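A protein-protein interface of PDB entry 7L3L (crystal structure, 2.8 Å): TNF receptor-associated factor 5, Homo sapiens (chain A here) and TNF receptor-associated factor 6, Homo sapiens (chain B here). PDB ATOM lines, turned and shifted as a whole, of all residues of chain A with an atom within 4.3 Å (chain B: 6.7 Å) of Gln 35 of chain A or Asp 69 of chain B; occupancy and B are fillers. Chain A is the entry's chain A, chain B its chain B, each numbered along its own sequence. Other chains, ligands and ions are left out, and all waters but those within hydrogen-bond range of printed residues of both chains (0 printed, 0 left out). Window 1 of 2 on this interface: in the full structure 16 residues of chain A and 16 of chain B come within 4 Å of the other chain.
Among the printed residues, pairs that only touch across the chains: Gly 39 of chain A with Phe 71 of chain B (3.3 Å), Phe 72 of chain A with Pro 68 of chain B (3.4 Å), Phe 72 of chain A with Phe 67 of chain B (3.4 Å), Phe 72 of chain A with Gln 31 of chain B (3.5 Å), Gly 39 of chain A with Asn 70 of chain B (3.9 Å), Val 71 of chain A with Phe 67 of chain B (3.9 Å), Gln 35 of chain A with Pro 68 of chain B (3.9 Å) and His 40 of chain A with Arg 74 of chain B (3.9 Å).
Gln 35 of chain A touches four residues of chain B.
Of the printed residues of chain B, Gly 39 of chain A touches Asn 70 (3.9 Å), Phe 71 (3.3 Å) and Arg 74 (2.2 Å).
Of the printed residues of chain A, Arg 74 of chain B touches Gly 39 (2.2 Å) and His 40 (3.9 Å).
The nearest residue of chain B that does not touch Gln 35 of chain A is Gln 31 of chain B (4.6 Å).
The nearest printed residue of chain A that does not touch Asp 69 of chain B is Phe 72 of chain A (4.4 Å).
The backbone carbonyl oxygen of Gly 39 of chain A lies close to the guanidinium group of Arg 74 of chain B (2.2 Å).
The side-chain amide nitrogen (NE2) of Gln 35 of chain A lies within hydrogen-bond range of the side-chain carboxylate (OD1) of Asp 69 of chain B, at 3.2 Å.
N of Asn 70 of chain B is in hydrogen-bond range of OE1 of Gln 35 of chain A (2.8 Å).
OE1 of Gln 35 of chain A lies within hydrogen-bond range of N of Phe 71 of chain B.
The side-chain carboxylate (OD1) of Asp 74 of chain A sits at hydrogen-bond distance from the side-chain amide nitrogen (NE2) of Gln 31 of chain B (2.7 Å).
Printed residues of chain B that touch a printed residue of chain A: Gln 31, Phe 67, Pro 68, Asp 69, Asn 70, Phe 71 and Arg 74.
Hydrophobic or aromatic side chains of chain B that line the printed part of chain A: Phe 67 and Phe 71.
Of the 9 printed residues of chain A, 6 touch a printed residue of chain B.
Hydrophobic or aromatic side chains of chain A within 4 Å of the printed part of chain B: His 40 and Phe 72.
Among the printed residues, no Asp or Glu carboxylate lies within 4 Å of a Lys or Arg side-chain nitrogen of the other chain.
The side-chain amide nitrogen of Gln 35 of chain A sits at hydrogen-bond distance from the side-chain carboxylate of Asp 74 of chain A, 3.0 Å away.
The side-chain amide oxygen (OD1) of Asn 70 of chain B lies within hydrogen-bond range of the side-chain amino group (NZ) of Lys 73 of chain B, 2.6 Å away.
The backbone carbonyl oxygen (O) of Ala 29 of chain B sits at hydrogen-bond distance from the backbone NH (N) of Asp 69 of chain B (2.9 Å).
NE of Arg 37 of chain B lies within salt-bridge range of OD2 of Asp 69 of chain B (3.0 Å).
The side-chain carboxylate (OD1) of Asp 69 of chain B sits close to the backbone NH (N) of Phe 71 of chain B (3.4 Å).
The backbone carbonyl oxygen (O) of His 40 of chain A lies within hydrogen-bond range of the side-chain hydroxyl (OG1) of Thr 36 of chain A (3.3 Å).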
ATOM      1  N   HIS A  34     -28.775 -28.052  15.652  1.00  0.00           N
ATOM      2  CA  HIS A  34     -27.975 -28.089  16.863  1.00  0.00           C
ATOM      3  C   HIS A  34     -27.218 -26.780  16.973  1.00  0.00           C
ATOM      4  O   HIS A  34     -26.715 -26.259  15.975  1.00  0.00           O
ATOM      5  CB  HIS A  34     -26.976 -29.245  16.866  1.00  0.00           C
ATOM      6  CG  HIS A  34     -27.610 -30.596  16.835  1.00  0.00           C
ATOM      7  ND1 HIS A  34     -28.533 -30.965  15.882  1.00  0.00           N
ATOM      8  CD2 HIS A  34     -27.440 -31.675  17.634  1.00  0.00           C
ATOM      9  CE1 HIS A  34     -28.916 -32.208  16.104  1.00  0.00           C
ATOM     10  NE2 HIS A  34     -28.264 -32.664  17.157  1.00  0.00           N
ATOM     11  N   GLN A  35     -27.143 -26.251  18.182  1.00  0.00           N
ATOM     12  CA  GLN A  35     -26.318 -25.089  18.446  1.00  0.00           C
ATOM     13  C   GLN A  35     -25.012 -25.534  19.089  1.00  0.00           C
ATOM     14  O   GLN A  35     -24.965 -26.520  19.830  1.00  0.00           O
ATOM     15  CB  GLN A  35     -27.036 -24.088  19.349  1.00  0.00           C
ATOM     16  CG  GLN A  35     -26.194 -22.878  19.698  1.00  0.00           C
ATOM     17  CD  GLN A  35     -26.971 -21.831  20.443  1.00  0.00           C
ATOM     18  OE1 GLN A  35     -26.406 -21.040  21.199  1.00  0.00           O
ATOM     19  NE2 GLN A  35     -28.281 -21.814  20.236  1.00  0.00           N
ATOM     20  N   THR A  36     -23.951 -24.806  18.778  1.00  0.00           N
ATOM     21  CA  THR A  36     -22.628 -25.055  19.316  1.00  0.00           C
ATOM     22  C   THR A  36     -22.297 -23.997  20.360  1.00  0.00           C
ATOM     23  O   THR A  36     -23.009 -23.001  20.515  1.00  0.00           O
ATOM     24  CB  THR A  36     -21.590 -25.055  18.192  1.00  0.00           C
ATOM     25  OG1 THR A  36     -21.611 -23.784  17.530  1.00  0.00           O
ATOM     26  CG2 THR A  36     -21.921 -26.141  17.181  1.00  0.00           C
ATOM     27  N   GLY A  39     -22.307 -20.331  19.431  1.00  0.00           N
ATOM     28  CA  GLY A  39     -23.544 -19.632  19.159  1.00  0.00           C
ATOM     29  C   GLY A  39     -23.961 -19.718  17.708  1.00  0.00           C
ATOM     30  O   GLY A  39     -24.463 -18.745  17.139  1.00  0.00           O
ATOM     31  N   HIS A  40     -23.759 -20.878  17.092  1.00  0.00           N
ATOM     32  CA  HIS A  40     -24.083 -21.072  15.689  1.00  0.00           C
ATOM     33  C   HIS A  40     -24.837 -22.378  15.511  1.00  0.00           C
ATOM     34  O   HIS A  40     -24.607 -23.351  16.234  1.00  0.00           O
ATOM     35  CB  HIS A  40     -22.821 -21.046  14.815  1.00  0.00           C
ATOM     36  CG  HIS A  40     -22.299 -19.665  14.574  1.00  0.00           C
ATOM     37  ND1 HIS A  40     -21.174 -19.172  15.196  1.00  0.00           N
ATOM     38  CD2 HIS A  40     -22.774 -18.659  13.802  1.00  0.00           C
ATOM     39  CE1 HIS A  40     -20.975 -17.922  14.814  1.00  0.00           C
ATOM     40  NE2 HIS A  40     -21.927 -17.590  13.962  1.00  0.00           N
ATOM     41  N   GLU A  70     -20.119 -28.921  24.501  1.00  0.00           N
ATOM     42  CA  GLU A  70     -20.925 -27.710  24.511  1.00  0.00           C
ATOM     43  C   GLU A  70     -21.915 -27.644  23.354  1.00  0.00           C
ATOM     44  O   GLU A  70     -22.580 -26.618  23.182  1.00  0.00           O
ATOM     45  CB  GLU A  70     -20.017 -26.480  24.503  1.00  0.00           C
ATOM     46  CG  GLU A  70     -19.169 -26.352  25.760  1.00  0.00           C
ATOM     47  CD  GLU A  70     -18.202 -25.187  25.704  1.00  0.00           C
ATOM     48  OE1 GLU A  70     -18.279 -24.389  24.746  1.00  0.00           O
ATOM     49  OE2 GLU A  70     -17.361 -25.070  26.620  1.00  0.00           O
ATOM     50  N   VAL A  71     -22.029 -28.706  22.567  1.00  0.00           N
ATOM     51  CA  VAL A  71     -23.001 -28.795  21.483  1.00  0.00           C
ATOM     52  C   VAL A  71     -24.310 -29.329  22.044  1.00  0.00           C
ATOM     53  O   VAL A  71     -24.309 -30.273  22.843  1.00  0.00           O
ATOM     54  CB  VAL A  71     -22.470 -29.702  20.355  1.00  0.00           C
ATOM     55  CG1 VAL A  71     -23.543 -29.955  19.303  1.00  0.00           C
ATOM     56  CG2 VAL A  71     -21.240 -29.095  19.730  1.00  0.00           C
ATOM     57  N   PHE A  72     -25.433 -28.736  21.635  1.00  0.00           N
ATOM     58  CA  PHE A  72     -26.725 -29.226  22.098  1.00  0.00           C
ATOM     59  C   PHE A  72     -27.768 -29.080  21.003  1.00  0.00           C
ATOM     60  O   PHE A  72     -27.621 -28.281  20.075  1.00  0.00           O
ATOM     61  CB  PHE A  72     -27.184 -28.510  23.375  1.00  0.00           C
ATOM     62  CG  PHE A  72     -27.497 -27.044  23.192  1.00  0.00           C
ATOM     63  CD1 PHE A  72     -26.482 -26.100  23.144  1.00  0.00           C
ATOM     64  CD2 PHE A  72     -28.812 -26.605  23.112  1.00  0.00           C
ATOM     65  CE1 PHE A  72     -26.775 -24.757  23.002  1.00  0.00           C
ATOM     66  CE2 PHE A  72     -29.107 -25.262  22.969  1.00  0.00           C
ATOM     67  CZ  PHE A  72     -28.089 -24.340  22.913  1.00  0.00           C
ATOM     68  N   ASP A  74     -30.896 -27.729  19.354  1.00  0.00           N
ATOM     69  CA  ASP A  74     -31.659 -26.484  19.438  1.00  0.00           C
ATOM     70  C   ASP A  74     -33.134 -26.786  19.174  1.00  0.00           C
ATOM     71  O   ASP A  74     -33.698 -26.484  18.121  1.00  0.00           O
ATOM     72  CB  ASP A  74     -31.109 -25.449  18.469  1.00  0.00           C
ATOM     73  CG  ASP A  74     -31.223 -24.042  19.007  1.00  0.00           C
ATOM     74  OD1 ASP A  74     -32.152 -23.791  19.801  1.00  0.00           O
ATOM     75  OD2 ASP A  74     -30.388 -23.189  18.642  1.00  0.00           O
ATOM     76  N   TYR B  17     -37.604 -13.989  22.471  1.00  0.00           N
ATOM     77  CA  TYR B  17     -36.482 -13.560  23.298  1.00  0.00           C
ATOM     78  C   TYR B  17     -36.943 -12.974  24.628  1.00  0.00           C
ATOM     79  O   TYR B  17     -36.218 -12.186  25.243  1.00  0.00           O
ATOM     80  CB  TYR B  17     -35.616 -12.553  22.540  1.00  0.00           C
ATOM     81  CG  TYR B  17     -35.017 -13.111  21.272  1.00  0.00           C
ATOM     82  CD1 TYR B  17     -34.604 -14.434  21.207  1.00  0.00           C
ATOM     83  CD2 TYR B  17     -34.865 -12.320  20.142  1.00  0.00           C
ATOM     84  CE1 TYR B  17     -34.056 -14.957  20.052  1.00  0.00           C
ATOM     85  CE2 TYR B  17     -34.317 -12.833  18.981  1.00  0.00           C
ATOM     86  CZ  TYR B  17     -33.915 -14.154  18.943  1.00  0.00           C
ATOM     87  OH  TYR B  17     -33.369 -14.674  17.793  1.00  0.00           O
ATOM     88  N   LEU B  26     -34.019 -11.973  27.864  1.00  0.00           N
ATOM     89  CA  LEU B  26     -33.215 -12.977  28.547  1.00  0.00           C
ATOM     90  C   LEU B  26     -31.834 -12.437  28.889  1.00  0.00           C
ATOM     91  O   LEU B  26     -31.159 -11.837  28.047  1.00  0.00           O
ATOM     92  CB  LEU B  26     -33.089 -14.219  27.668  1.00  0.00           C
ATOM     93  CG  LEU B  26     -34.390 -14.762  27.087  1.00  0.00           C
ATOM     94  CD1 LEU B  26     -34.129 -15.499  25.796  1.00  0.00           C
ATOM     95  CD2 LEU B  26     -35.047 -15.677  28.082  1.00  0.00           C
ATOM     96  N   GLU B  28     -28.167 -13.636  30.047  1.00  0.00           N
ATOM     97  CA  GLU B  28     -27.385 -14.868  29.954  1.00  0.00           C
ATOM     98  C   GLU B  28     -28.317 -16.061  29.714  1.00  0.00           C
ATOM     99  O   GLU B  28     -28.494 -16.946  30.550  1.00  0.00           O
ATOM    100  CB  GLU B  28     -26.512 -15.062  31.198  1.00  0.00           C
ATOM    101  CG  GLU B  28     -25.187 -14.296  31.154  1.00  0.00           C
ATOM    102  CD  GLU B  28     -24.330 -14.644  29.940  1.00  0.00           C
ATOM    103  OE1 GLU B  28     -24.244 -15.841  29.587  1.00  0.00           O
ATOM    104  OE2 GLU B  28     -23.737 -13.719  29.342  1.00  0.00           O
ATOM    105  N   ALA B  29     -28.938 -16.021  28.539  1.00  0.00           N
ATOM    106  CA  ALA B  29     -30.007 -16.951  28.209  1.00  0.00           C
ATOM    107  C   ALA B  29     -29.517 -18.394  28.189  1.00  0.00           C
ATOM    108  O   ALA B  29     -28.386 -18.683  27.789  1.00  0.00           O
ATOM    109  CB  ALA B  29     -30.614 -16.592  26.853  1.00  0.00           C
ATOM    110  N   VAL B  30     -30.392 -19.299  28.625  1.00  0.00           N
ATOM    111  CA  VAL B  30     -30.161 -20.736  28.584  1.00  0.00           C
ATOM    112  C   VAL B  30     -31.401 -21.399  28.000  1.00  0.00           C
ATOM    113  O   VAL B  30     -32.509 -20.864  28.081  1.00  0.00           O
ATOM    114  CB  VAL B  30     -29.842 -21.308  29.983  1.00  0.00           C
ATOM    115  CG1 VAL B  30     -28.633 -20.607  30.582  1.00  0.00           C
ATOM    116  CG2 VAL B  30     -31.048 -21.169  30.899  1.00  0.00           C
ATOM    117  N   GLN B  31     -31.210 -22.574  27.405  1.00  0.00           N
ATOM    118  CA  GLN B  31     -32.288 -23.313  26.766  1.00  0.00           C
ATOM    119  C   GLN B  31     -32.440 -24.678  27.423  1.00  0.00           C
ATOM    120  O   GLN B  31     -31.462 -25.275  27.881  1.00  0.00           O
ATOM    121  CB  GLN B  31     -32.027 -23.480  25.259  1.00  0.00           C
ATOM    122  CG  GLN B  31     -33.184 -24.080  24.469  1.00  0.00           C
ATOM    123  CD  GLN B  31     -32.885 -24.198  22.984  1.00  0.00           C
ATOM    124  OE1 GLN B  31     -33.472 -25.020  22.283  1.00  0.00           O
ATOM    125  NE2 GLN B  31     -31.969 -23.369  22.499  1.00  0.00           N
ATOM    126  N   ARG B  37     -36.586 -20.981  26.442  1.00  0.00           N
ATOM    127  CA  ARG B  37     -35.486 -20.136  26.880  1.00  0.00           C
ATOM    128  C   ARG B  37     -35.869 -19.398  28.156  1.00  0.00           C
ATOM    129  O   ARG B  37     -37.007 -18.953  28.309  1.00  0.00           O
ATOM    130  CB  ARG B  37     -35.106 -19.131  25.790  1.00  0.00           C
ATOM    131  CG  ARG B  37     -34.865 -19.756  24.420  1.00  0.00           C
ATOM    132  CD  ARG B  37     -34.401 -18.714  23.403  1.00  0.00           C
ATOM    133  NE  ARG B  37     -33.990 -19.323  22.137  1.00  0.00           N
ATOM    134  CZ  ARG B  37     -34.709 -19.294  21.019  1.00  0.00           C
ATOM    135  NH1 ARG B  37     -35.887 -18.681  20.999  1.00  0.00           N
ATOM    136  NH2 ARG B  37     -34.253 -19.880  19.919  1.00  0.00           N
ATOM    137  N   PHE B  67     -28.295 -25.718  28.644  1.00  0.00           N
ATOM    138  CA  PHE B  67     -27.186 -25.253  27.841  1.00  0.00           C
ATOM    139  C   PHE B  67     -27.308 -23.754  27.612  1.00  0.00           C
ATOM    140  O   PHE B  67     -28.424 -23.246  27.457  1.00  0.00           O
ATOM    141  CB  PHE B  67     -27.146 -25.973  26.491  1.00  0.00           C
ATOM    142  CG  PHE B  67     -26.570 -27.357  26.561  1.00  0.00           C
ATOM    143  CD1 PHE B  67     -25.220 -27.574  26.339  1.00  0.00           C
ATOM    144  CD2 PHE B  67     -27.376 -28.442  26.854  1.00  0.00           C
ATOM    145  CE1 PHE B  67     -24.688 -28.848  26.407  1.00  0.00           C
ATOM    146  CE2 PHE B  67     -26.847 -29.717  26.921  1.00  0.00           C
ATOM    147  CZ  PHE B  67     -25.504 -29.918  26.699  1.00  0.00           C
ATOM    148  N   PRO B  68     -26.202 -23.016  27.605  1.00  0.00           N
ATOM    149  CA  PRO B  68     -26.289 -21.587  27.290  1.00  0.00           C
ATOM    150  C   PRO B  68     -26.692 -21.386  25.838  1.00  0.00           C
ATOM    151  O   PRO B  68     -26.203 -22.073  24.937  1.00  0.00           O
ATOM    152  CB  PRO B  68     -24.871 -21.071  27.564  1.00  0.00           C
ATOM    153  CG  PRO B  68     -23.999 -22.268  27.429  1.00  0.00           C
ATOM    154  CD  PRO B  68     -24.818 -23.443  27.881  1.00  0.00           C
ATOM    155  N   ASP B  69     -27.614 -20.450  25.619  1.00  0.00           N
ATOM    156  CA  ASP B  69     -28.105 -20.146  24.276  1.00  0.00           C
ATOM    157  C   ASP B  69     -27.380 -18.895  23.794  1.00  0.00           C
ATOM    158  O   ASP B  69     -27.865 -17.770  23.911  1.00  0.00           O
ATOM    159  CB  ASP B  69     -29.619 -19.964  24.277  1.00  0.00           C
ATOM    160  CG  ASP B  69     -30.206 -19.958  22.880  1.00  0.00           C
ATOM    161  OD1 ASP B  69     -29.572 -19.395  21.964  1.00  0.00           O
ATOM    162  OD2 ASP B  69     -31.305 -20.519  22.693  1.00  0.00           O
ATOM    163  N   ASN B  70     -26.188 -19.107  23.241  1.00  0.00           N
ATOM    164  CA  ASN B  70     -25.357 -17.989  22.823  1.00  0.00           C
ATOM    165  C   ASN B  70     -25.766 -17.416  21.473  1.00  0.00           C
ATOM    166  O   ASN B  70     -25.246 -16.363  21.087  1.00  0.00           O
ATOM    167  CB  ASN B  70     -23.890 -18.420  22.798  1.00  0.00           C
ATOM    168  CG  ASN B  70     -23.370 -18.772  24.180  1.00  0.00           C
ATOM    169  OD1 ASN B  70     -23.296 -17.920  25.062  1.00  0.00           O
ATOM    170  ND2 ASN B  70     -23.016 -20.035  24.374  1.00  0.00           N
ATOM    171  N   PHE B  71     -26.681 -18.069  20.752  1.00  0.00           N
ATOM    172  CA  PHE B  71     -27.238 -17.462  19.547  1.00  0.00           C
ATOM    173  C   PHE B  71     -28.236 -16.372  19.904  1.00  0.00           C
ATOM    174  O   PHE B  71     -28.208 -15.282  19.324  1.00  0.00           O
ATOM    175  CB  PHE B  71     -27.904 -18.518  18.666  1.00  0.00           C
ATOM    176  CG  PHE B  71     -28.347 -17.998  17.324  1.00  0.00           C
ATOM    177  CD1 PHE B  71     -29.536 -17.299  17.190  1.00  0.00           C
ATOM    178  CD2 PHE B  71     -27.575 -18.212  16.195  1.00  0.00           C
ATOM    179  CE1 PHE B  71     -29.942 -16.819  15.962  1.00  0.00           C
ATOM    180  CE2 PHE B  71     -27.979 -17.736  14.960  1.00  0.00           C
ATOM    181  CZ  PHE B  71     -29.165 -17.041  14.845  1.00  0.00           C
ATOM    182  N   ALA B  72     -29.140 -16.658  20.841  1.00  0.00           N
ATOM    183  CA  ALA B  72     -30.071 -15.636  21.299  1.00  0.00           C
ATOM    184  C   ALA B  72     -29.350 -14.551  22.090  1.00  0.00           C
ATOM    185  O   ALA B  72     -29.652 -13.361  21.934  1.00  0.00           O
ATOM    186  CB  ALA B  72     -31.177 -16.270  22.142  1.00  0.00           C
ATOM    187  N   LYS B  73     -28.394 -14.938  22.942  1.00  0.00           N
ATOM    188  CA  LYS B  73     -27.652 -13.951  23.719  1.00  0.00           C
ATOM    189  C   LYS B  73     -26.980 -12.927  22.812  1.00  0.00           C
ATOM    190  O   LYS B  73     -26.908 -11.740  23.150  1.00  0.00           O
ATOM    191  CB  LYS B  73     -26.616 -14.643  24.607  1.00  0.00           C
ATOM    192  CG  LYS B  73     -25.892 -13.682  25.541  1.00  0.00           C
ATOM    193  CD  LYS B  73     -24.402 -13.958  25.608  1.00  0.00           C
ATOM    194  CE  LYS B  73     -24.113 -15.234  26.378  1.00  0.00           C
ATOM    195  NZ  LYS B  73     -22.707 -15.702  26.188  1.00  0.00           N
ATOM    196  N   ARG B  74     -26.496 -13.363  21.649  1.00  0.00           N
ATOM    197  CA  ARG B  74     -25.905 -12.423  20.705  1.00  0.00           C
ATOM    198  C   ARG B  74     -26.969 -11.530  20.081  1.00  0.00           C
ATOM    199  O   ARG B  74     -26.827 -10.303  20.061  1.00  0.00           O
ATOM    200  CB  ARG B  74     -25.129 -13.174  19.623  1.00  0.00           C
ATOM    201  CG  ARG B  74     -24.160 -12.287  18.851  1.00  0.00           C
ATOM    202  CD  ARG B  74     -23.183 -13.102  18.017  1.00  0.00           C
ATOM    203  NE  ARG B  74     -23.771 -14.355  17.555  1.00  0.00           N
ATOM    204  CZ  ARG B  74     -23.203 -15.545  17.717  1.00  0.00           C
ATOM    205  NH1 ARG B  74     -22.031 -15.641  18.330  1.00  0.00           N
ATOM    206  NH2 ARG B  74     -23.809 -16.634  17.265  1.00  0.00           N
